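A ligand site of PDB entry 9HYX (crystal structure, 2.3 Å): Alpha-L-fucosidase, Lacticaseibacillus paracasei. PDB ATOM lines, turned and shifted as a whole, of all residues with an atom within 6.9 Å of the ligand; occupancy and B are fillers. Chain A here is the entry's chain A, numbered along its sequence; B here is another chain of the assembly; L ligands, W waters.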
ATOM      1  N   PHE A  19      25.775 -12.821 -17.406  1.00  0.00           N
ATOM      2  CA  PHE A  19      25.088 -14.096 -17.527  1.00  0.00           C
ATOM      3  C   PHE A  19      25.219 -14.820 -16.181  1.00  0.00           C
ATOM      4  O   PHE A  19      26.310 -14.868 -15.624  1.00  0.00           O
ATOM      5  CB  PHE A  19      25.812 -14.874 -18.624  1.00  0.00           C
ATOM      6  CG  PHE A  19      25.001 -15.817 -19.499  1.00  0.00           C
ATOM      7  CD1 PHE A  19      23.777 -16.352 -19.059  1.00  0.00           C
ATOM      8  CD2 PHE A  19      25.468 -16.159 -20.774  1.00  0.00           C
ATOM      9  CE1 PHE A  19      23.051 -17.215 -19.882  1.00  0.00           C
ATOM     10  CE2 PHE A  19      24.746 -17.013 -21.592  1.00  0.00           C
ATOM     11  CZ  PHE A  19      23.526 -17.547 -21.136  1.00  0.00           C
ATOM     12  N   HIS A  21      24.450 -18.550 -14.387  1.00  0.00           N
ATOM     13  CA  HIS A  21      24.037 -19.944 -14.374  1.00  0.00           C
ATOM     14  C   HIS A  21      23.883 -20.381 -12.913  1.00  0.00           C
ATOM     15  O   HIS A  21      24.851 -20.355 -12.133  1.00  0.00           O
ATOM     16  CB  HIS A  21      25.047 -20.858 -15.079  1.00  0.00           C
ATOM     17  CG  HIS A  21      24.929 -20.781 -16.567  1.00  0.00           C
ATOM     18  ND1 HIS A  21      25.223 -19.629 -17.279  1.00  0.00           N
ATOM     19  CD2 HIS A  21      24.460 -21.682 -17.468  1.00  0.00           C
ATOM     20  CE1 HIS A  21      24.964 -19.854 -18.573  1.00  0.00           C
ATOM     21  NE2 HIS A  21      24.467 -21.075 -18.707  1.00  0.00           N
ATOM     22  N   GLU A  32      27.297 -27.580 -15.373  1.00  0.00           N
ATOM     23  CA  GLU A  32      25.853 -27.572 -15.495  1.00  0.00           C
ATOM     24  C   GLU A  32      25.338 -28.782 -16.296  1.00  0.00           C
ATOM     25  O   GLU A  32      24.179 -29.144 -16.181  1.00  0.00           O
ATOM     26  CB  GLU A  32      25.345 -26.241 -16.070  1.00  0.00           C
ATOM     27  CG  GLU A  32      25.672 -26.015 -17.552  1.00  0.00           C
ATOM     28  CD  GLU A  32      27.115 -25.716 -17.957  1.00  0.00           C
ATOM     29  OE1 GLU A  32      28.036 -25.636 -17.077  1.00  0.00           O
ATOM     30  OE2 GLU A  32      27.362 -25.567 -19.197  1.00  0.00           O
ATOM     31  N   TRP A  33      26.188 -29.417 -17.122  1.00  0.00           N
ATOM     32  CA  TRP A  33      25.772 -30.602 -17.870  1.00  0.00           C
ATOM     33  C   TRP A  33      25.943 -31.891 -17.060  1.00  0.00           C
ATOM     34  O   TRP A  33      25.838 -32.966 -17.631  1.00  0.00           O
ATOM     35  CB  TRP A  33      26.538 -30.702 -19.194  1.00  0.00           C
ATOM     36  CG  TRP A  33      25.937 -29.903 -20.323  1.00  0.00           C
ATOM     37  CD1 TRP A  33      25.898 -28.544 -20.441  1.00  0.00           C
ATOM     38  CD2 TRP A  33      25.347 -30.437 -21.528  1.00  0.00           C
ATOM     39  NE1 TRP A  33      25.286 -28.186 -21.619  1.00  0.00           N
ATOM     40  CE2 TRP A  33      24.971 -29.330 -22.322  1.00  0.00           C
ATOM     41  CE3 TRP A  33      25.121 -31.732 -22.015  1.00  0.00           C
ATOM     42  CZ2 TRP A  33      24.364 -29.483 -23.573  1.00  0.00           C
ATOM     43  CZ3 TRP A  33      24.525 -31.881 -23.257  1.00  0.00           C
ATOM     44  CH2 TRP A  33      24.167 -30.777 -24.037  1.00  0.00           C
ATOM     45  N   THR A  77      19.451 -18.012 -15.766  1.00  0.00           N
ATOM     46  CA  THR A  77      18.918 -19.310 -16.167  1.00  0.00           C
ATOM     47  C   THR A  77      17.615 -19.562 -15.408  1.00  0.00           C
ATOM     48  O   THR A  77      17.662 -19.806 -14.193  1.00  0.00           O
ATOM     49  CB  THR A  77      19.938 -20.428 -15.890  1.00  0.00           C
ATOM     50  OG1 THR A  77      20.361 -20.299 -14.528  1.00  0.00           O
ATOM     51  CG2 THR A  77      21.138 -20.401 -16.829  1.00  0.00           C
ATOM     52  N   HIS A  80      17.344 -24.687 -17.020  1.00  0.00           N
ATOM     53  CA  HIS A  80      18.424 -25.220 -17.845  1.00  0.00           C
ATOM     54  C   HIS A  80      18.029 -26.623 -18.350  1.00  0.00           C
ATOM     55  O   HIS A  80      16.915 -27.060 -18.127  1.00  0.00           O
ATOM     56  CB  HIS A  80      19.765 -25.086 -17.082  1.00  0.00           C
ATOM     57  CG  HIS A  80      20.942 -25.020 -17.980  1.00  0.00           C
ATOM     58  ND1 HIS A  80      21.608 -26.149 -18.437  1.00  0.00           N
ATOM     59  CD2 HIS A  80      21.532 -23.953 -18.574  1.00  0.00           C
ATOM     60  CE1 HIS A  80      22.568 -25.772 -19.305  1.00  0.00           C
ATOM     61  NE2 HIS A  80      22.548 -24.422 -19.397  1.00  0.00           N
ATOM     62  N   HIS A  81      18.940 -27.335 -19.030  1.00  0.00           N
ATOM     63  CA  HIS A  81      18.620 -28.654 -19.553  1.00  0.00           C
ATOM     64  C   HIS A  81      18.065 -29.590 -18.468  1.00  0.00           C
ATOM     65  O   HIS A  81      17.209 -30.427 -18.753  1.00  0.00           O
ATOM     66  CB  HIS A  81      19.820 -29.308 -20.246  1.00  0.00           C
ATOM     67  CG  HIS A  81      20.432 -28.460 -21.304  1.00  0.00           C
ATOM     68  ND1 HIS A  81      19.699 -27.868 -22.291  1.00  0.00           N
ATOM     69  CD2 HIS A  81      21.709 -28.120 -21.549  1.00  0.00           C
ATOM     70  CE1 HIS A  81      20.505 -27.194 -23.108  1.00  0.00           C
ATOM     71  NE2 HIS A  81      21.720 -27.314 -22.661  1.00  0.00           N
ATOM     72  N   TYR A 124      16.891 -16.743 -19.454  1.00  0.00           N
ATOM     73  CA  TYR A 124      17.382 -17.825 -20.274  1.00  0.00           C
ATOM     74  C   TYR A 124      16.406 -18.994 -20.114  1.00  0.00           C
ATOM     75  O   TYR A 124      15.975 -19.293 -18.988  1.00  0.00           O
ATOM     76  CB  TYR A 124      18.794 -18.165 -19.806  1.00  0.00           C
ATOM     77  CG  TYR A 124      19.304 -19.516 -20.306  1.00  0.00           C
ATOM     78  CD1 TYR A 124      18.765 -20.703 -19.809  1.00  0.00           C
ATOM     79  CD2 TYR A 124      20.318 -19.579 -21.261  1.00  0.00           C
ATOM     80  CE1 TYR A 124      19.217 -21.929 -20.266  1.00  0.00           C
ATOM     81  CE2 TYR A 124      20.809 -20.817 -21.704  1.00  0.00           C
ATOM     82  CZ  TYR A 124      20.240 -21.975 -21.212  1.00  0.00           C
ATOM     83  OH  TYR A 124      20.647 -23.190 -21.652  1.00  0.00           O
ATOM     84  N   TRP A 164      16.254 -15.362 -23.650  1.00  0.00           N
ATOM     85  CA  TRP A 164      17.471 -15.888 -24.232  1.00  0.00           C
ATOM     86  C   TRP A 164      17.248 -17.382 -24.448  1.00  0.00           C
ATOM     87  O   TRP A 164      17.252 -18.172 -23.499  1.00  0.00           O
ATOM     88  CB  TRP A 164      18.623 -15.558 -23.260  1.00  0.00           C
ATOM     89  CG  TRP A 164      20.017 -15.485 -23.844  1.00  0.00           C
ATOM     90  CD1 TRP A 164      20.734 -14.338 -24.088  1.00  0.00           C
ATOM     91  CD2 TRP A 164      20.892 -16.582 -24.214  1.00  0.00           C
ATOM     92  NE1 TRP A 164      21.969 -14.639 -24.604  1.00  0.00           N
ATOM     93  CE2 TRP A 164      22.107 -16.005 -24.679  1.00  0.00           C
ATOM     94  CE3 TRP A 164      20.778 -17.981 -24.193  1.00  0.00           C
ATOM     95  CZ2 TRP A 164      23.186 -16.789 -25.106  1.00  0.00           C
ATOM     96  CZ3 TRP A 164      21.843 -18.754 -24.630  1.00  0.00           C
ATOM     97  CH2 TRP A 164      23.043 -18.173 -25.066  1.00  0.00           C
ATOM     98  N   ASP A 166      17.955 -21.032 -25.685  1.00  0.00           N
ATOM     99  CA  ASP A 166      19.044 -21.922 -26.011  1.00  0.00           C
ATOM    100  C   ASP A 166      18.492 -23.133 -26.752  1.00  0.00           C
ATOM    101  O   ASP A 166      17.942 -24.059 -26.116  1.00  0.00           O
ATOM    102  CB  ASP A 166      19.808 -22.277 -24.756  1.00  0.00           C
ATOM    103  CG  ASP A 166      20.979 -23.225 -24.968  1.00  0.00           C
ATOM    104  OD1 ASP A 166      21.306 -23.506 -26.122  1.00  0.00           O
ATOM    105  OD2 ASP A 166      21.532 -23.695 -23.967  1.00  0.00           O
ATOM    106  N   GLY A 167      18.677 -23.124 -28.088  1.00  0.00           N
ATOM    107  CA  GLY A 167      18.087 -24.143 -28.962  1.00  0.00           C
ATOM    108  C   GLY A 167      19.094 -25.172 -29.462  1.00  0.00           C
ATOM    109  O   GLY A 167      18.825 -25.885 -30.433  1.00  0.00           O
ATOM    110  N   ASN A 168      20.263 -25.243 -28.788  1.00  0.00           N
ATOM    111  CA  ASN A 168      21.333 -26.167 -29.146  1.00  0.00           C
ATOM    112  C   ASN A 168      21.001 -27.579 -28.673  1.00  0.00           C
ATOM    113  O   ASN A 168      20.213 -27.751 -27.741  1.00  0.00           O
ATOM    114  CB  ASN A 168      22.579 -25.801 -28.375  1.00  0.00           C
ATOM    115  CG  ASN A 168      23.384 -24.740 -29.074  1.00  0.00           C
ATOM    116  OD1 ASN A 168      23.136 -24.436 -30.253  1.00  0.00           O
ATOM    117  ND2 ASN A 168      24.357 -24.174 -28.384  1.00  0.00           N
ATOM    118  N   TRP A 169      21.624 -28.575 -29.328  1.00  0.00           N
ATOM    119  CA  TRP A 169      21.535 -29.985 -28.974  1.00  0.00           C
ATOM    120  C   TRP A 169      20.148 -30.613 -29.228  1.00  0.00           C
ATOM    121  O   TRP A 169      19.821 -31.674 -28.714  1.00  0.00           O
ATOM    122  CB  TRP A 169      22.136 -30.212 -27.592  1.00  0.00           C
ATOM    123  CG  TRP A 169      23.631 -30.219 -27.824  1.00  0.00           C
ATOM    124  CD1 TRP A 169      24.302 -31.124 -28.604  1.00  0.00           C
ATOM    125  CD2 TRP A 169      24.587 -29.195 -27.495  1.00  0.00           C
ATOM    126  NE1 TRP A 169      25.626 -30.779 -28.712  1.00  0.00           N
ATOM    127  CE2 TRP A 169      25.834 -29.610 -28.034  1.00  0.00           C
ATOM    128  CE3 TRP A 169      24.540 -28.024 -26.717  1.00  0.00           C
ATOM    129  CZ2 TRP A 169      27.009 -28.861 -27.855  1.00  0.00           C
ATOM    130  CZ3 TRP A 169      25.700 -27.286 -26.551  1.00  0.00           C
ATOM    131  CH2 TRP A 169      26.911 -27.696 -27.117  1.00  0.00           C
ATOM    132  N   ASN A 197      20.310 -18.518 -29.585  1.00  0.00           N
ATOM    133  CA  ASN A 197      21.659 -19.000 -29.896  1.00  0.00           C
ATOM    134  C   ASN A 197      21.682 -19.956 -31.095  1.00  0.00           C
ATOM    135  O   ASN A 197      22.710 -20.504 -31.444  1.00  0.00           O
ATOM    136  CB  ASN A 197      22.428 -19.485 -28.674  1.00  0.00           C
ATOM    137  CG  ASN A 197      21.935 -20.859 -28.301  1.00  0.00           C
ATOM    138  OD1 ASN A 197      20.921 -21.324 -28.891  1.00  0.00           O
ATOM    139  ND2 ASN A 197      22.653 -21.521 -27.375  1.00  0.00           N
ATOM    140  N   SER A 239      29.499 -14.178 -25.784  1.00  0.00           N
ATOM    141  CA  SER A 239      29.484 -14.654 -24.415  1.00  0.00           C
ATOM    142  C   SER A 239      30.872 -15.118 -24.038  1.00  0.00           C
ATOM    143  O   SER A 239      31.596 -15.660 -24.865  1.00  0.00           O
ATOM    144  CB  SER A 239      28.580 -15.842 -24.305  1.00  0.00           C
ATOM    145  OG  SER A 239      27.265 -15.347 -24.193  1.00  0.00           O
ATOM    146  N   TRP A 246      30.037 -23.236 -17.539  1.00  0.00           N
ATOM    147  CA  TRP A 246      29.094 -22.150 -17.322  1.00  0.00           C
ATOM    148  C   TRP A 246      28.522 -22.197 -15.904  1.00  0.00           C
ATOM    149  O   TRP A 246      28.493 -21.176 -15.228  1.00  0.00           O
ATOM    150  CB  TRP A 246      27.985 -22.208 -18.390  1.00  0.00           C
ATOM    151  CG  TRP A 246      28.558 -22.029 -19.760  1.00  0.00           C
ATOM    152  CD1 TRP A 246      29.136 -22.993 -20.531  1.00  0.00           C
ATOM    153  CD2 TRP A 246      28.724 -20.770 -20.473  1.00  0.00           C
ATOM    154  NE1 TRP A 246      29.630 -22.445 -21.680  1.00  0.00           N
ATOM    155  CE2 TRP A 246      29.395 -21.083 -21.679  1.00  0.00           C
ATOM    156  CE3 TRP A 246      28.358 -19.430 -20.220  1.00  0.00           C
ATOM    157  CZ2 TRP A 246      29.720 -20.108 -22.638  1.00  0.00           C
ATOM    158  CZ3 TRP A 246      28.637 -18.482 -21.182  1.00  0.00           C
ATOM    159  CH2 TRP A 246      29.362 -18.802 -22.348  1.00  0.00           C
ATOM    160  N   GLY A 247      28.049 -23.375 -15.456  1.00  0.00           N
ATOM    161  CA  GLY A 247      27.769 -23.538 -14.042  1.00  0.00           C
ATOM    162  C   GLY A 247      29.091 -23.642 -13.271  1.00  0.00           C
ATOM    163  O   GLY A 247      30.149 -23.887 -13.860  1.00  0.00           O
ATOM    164  N   ASN A 278      29.878 -14.379 -17.975  1.00  0.00           N
ATOM    165  CA  ASN A 278      29.120 -15.370 -17.242  1.00  0.00           C
ATOM    166  C   ASN A 278      29.698 -15.602 -15.853  1.00  0.00           C
ATOM    167  O   ASN A 278      30.911 -15.734 -15.712  1.00  0.00           O
ATOM    168  CB  ASN A 278      29.096 -16.718 -17.965  1.00  0.00           C
ATOM    169  CG  ASN A 278      28.388 -17.761 -17.127  1.00  0.00           C
ATOM    170  OD1 ASN A 278      27.169 -17.642 -16.909  1.00  0.00           O
ATOM    171  ND2 ASN A 278      29.103 -18.750 -16.602  1.00  0.00           N
ATOM    172  N   TYR B 400      34.490 -34.101 -17.242  1.00  0.00           N
ATOM    173  CA  TYR B 400      33.655 -32.926 -17.295  1.00  0.00           C
ATOM    174  C   TYR B 400      33.556 -32.337 -15.902  1.00  0.00           C
ATOM    175  O   TYR B 400      33.448 -33.067 -14.925  1.00  0.00           O
ATOM    176  CB  TYR B 400      32.278 -33.278 -17.884  1.00  0.00           C
ATOM    177  CG  TYR B 400      31.366 -32.057 -17.935  1.00  0.00           C
ATOM    178  CD1 TYR B 400      31.501 -31.101 -18.928  1.00  0.00           C
ATOM    179  CD2 TYR B 400      30.396 -31.866 -16.963  1.00  0.00           C
ATOM    180  CE1 TYR B 400      30.695 -29.977 -18.955  1.00  0.00           C
ATOM    181  CE2 TYR B 400      29.570 -30.761 -16.983  1.00  0.00           C
ATOM    182  CZ  TYR B 400      29.740 -29.804 -17.961  1.00  0.00           C
ATOM    183  OH  TYR B 400      28.912 -28.714 -17.973  1.00  0.00           O
HETATM  184  C1  LIG L   1      24.287 -23.390 -24.020  1.00  0.00           C
HETATM  185  C2  LIG L   1      24.332 -24.482 -22.942  1.00  0.00           C
HETATM  186  C3  LIG L   1      25.440 -24.272 -21.911  1.00  0.00           C
HETATM  187  C4  LIG L   1      25.399 -22.834 -21.448  1.00  0.00           C
HETATM  188  C5  LIG L   1      25.732 -21.925 -22.641  1.00  0.00           C
HETATM  189  C6  LIG L   1      25.117 -20.547 -22.480  1.00  0.00           C
HETATM  190  O1  LIG L   1      24.353 -24.008 -25.303  1.00  0.00           O
HETATM  191  O2  LIG L   1      24.460 -25.769 -23.540  1.00  0.00           O
HETATM  192  O3  LIG L   1      25.229 -25.136 -20.795  1.00  0.00           O
HETATM  193  O4  LIG L   1      24.089 -22.537 -20.976  1.00  0.00           O
HETATM  194  O5  LIG L   1      25.380 -22.466 -23.922  1.00  0.00           O
HETATM  195  O   HOH W   1      25.193 -21.025 -26.407  1.00  0.00           O
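O2 of the ligand is in hydrogen-bond range of NE2 of His 81, 3.3 Å away.
OD2 of Asp 166 sits close to O1 of the ligand, 3.1 Å away.
O4 of the ligand sits at hydrogen-bond distance from NE2 of His 80 (2.9 Å).
The side-chain carboxylate (OE2) of Glu 32 is in hydrogen-bond range of an oxygen (O3) of the ligand (2.7 Å).
O3 of the ligand is in hydrogen-bond range of NE1 of Trp 33 (3.2 Å).
An oxygen (O4) of the ligand is in hydrogen-bond range of a ring nitrogen (NE2) of His 21 (2.7 Å).
The side-chain amide nitrogen (ND2) of Asn 168 is in hydrogen-bond range of an oxygen (O1) of the ligand, 3.1 Å away.
ND1 of His 21 is in hydrogen-bond range of OD1 of Asn 278 (2.8 Å).
The backbone NH of Gly 247 is in hydrogen-bond range of the side-chain carboxylate of Glu 32 (2.8 Å).
The backbone carbonyl oxygen of Phe 19 sits close to the side-chain amide oxygen of Asn 278.
The side-chain carboxylate (OD2) of Asp 166 sits at hydrogen-bond distance from the side-chain hydroxyl (OH) of Tyr 124, at 2.5 Å.
OE1 of Glu 32 sits at hydrogen-bond distance from N of Trp 246 (3.2 Å).
NE2 of His 80 lies within hydrogen-bond range of OH of Tyr 124 (3.2 Å).
The side-chain hydroxyl of Tyr 400 of chain B lies within hydrogen-bond range of the backbone NH of Glu 32, 3.3 Å away.
ND2 of Asn 197 lies within hydrogen-bond range of OD1 of Asp 166 (2.7 Å).
Merely in contact with the ligand: Phe 19, Tyr 124, Trp 169, Asn 197 and Trp 246.
Hydrophobic or aromatic side chains that line the ligand: Phe 19, His 21, Trp 33, His 80, Tyr 124, Trp 169 and Trp 246.
Of the 19 residues printed, 12 come within 4 Å of the ligand.
The nearest printed residue that does not touch the ligand is Trp 164 (4.1 Å).
Water W1 lies within hydrogen-bond range of the side-chain amide nitrogen of Asn 197 (2.8 Å) and an oxygen (O5) of the ligand (2.9 Å).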
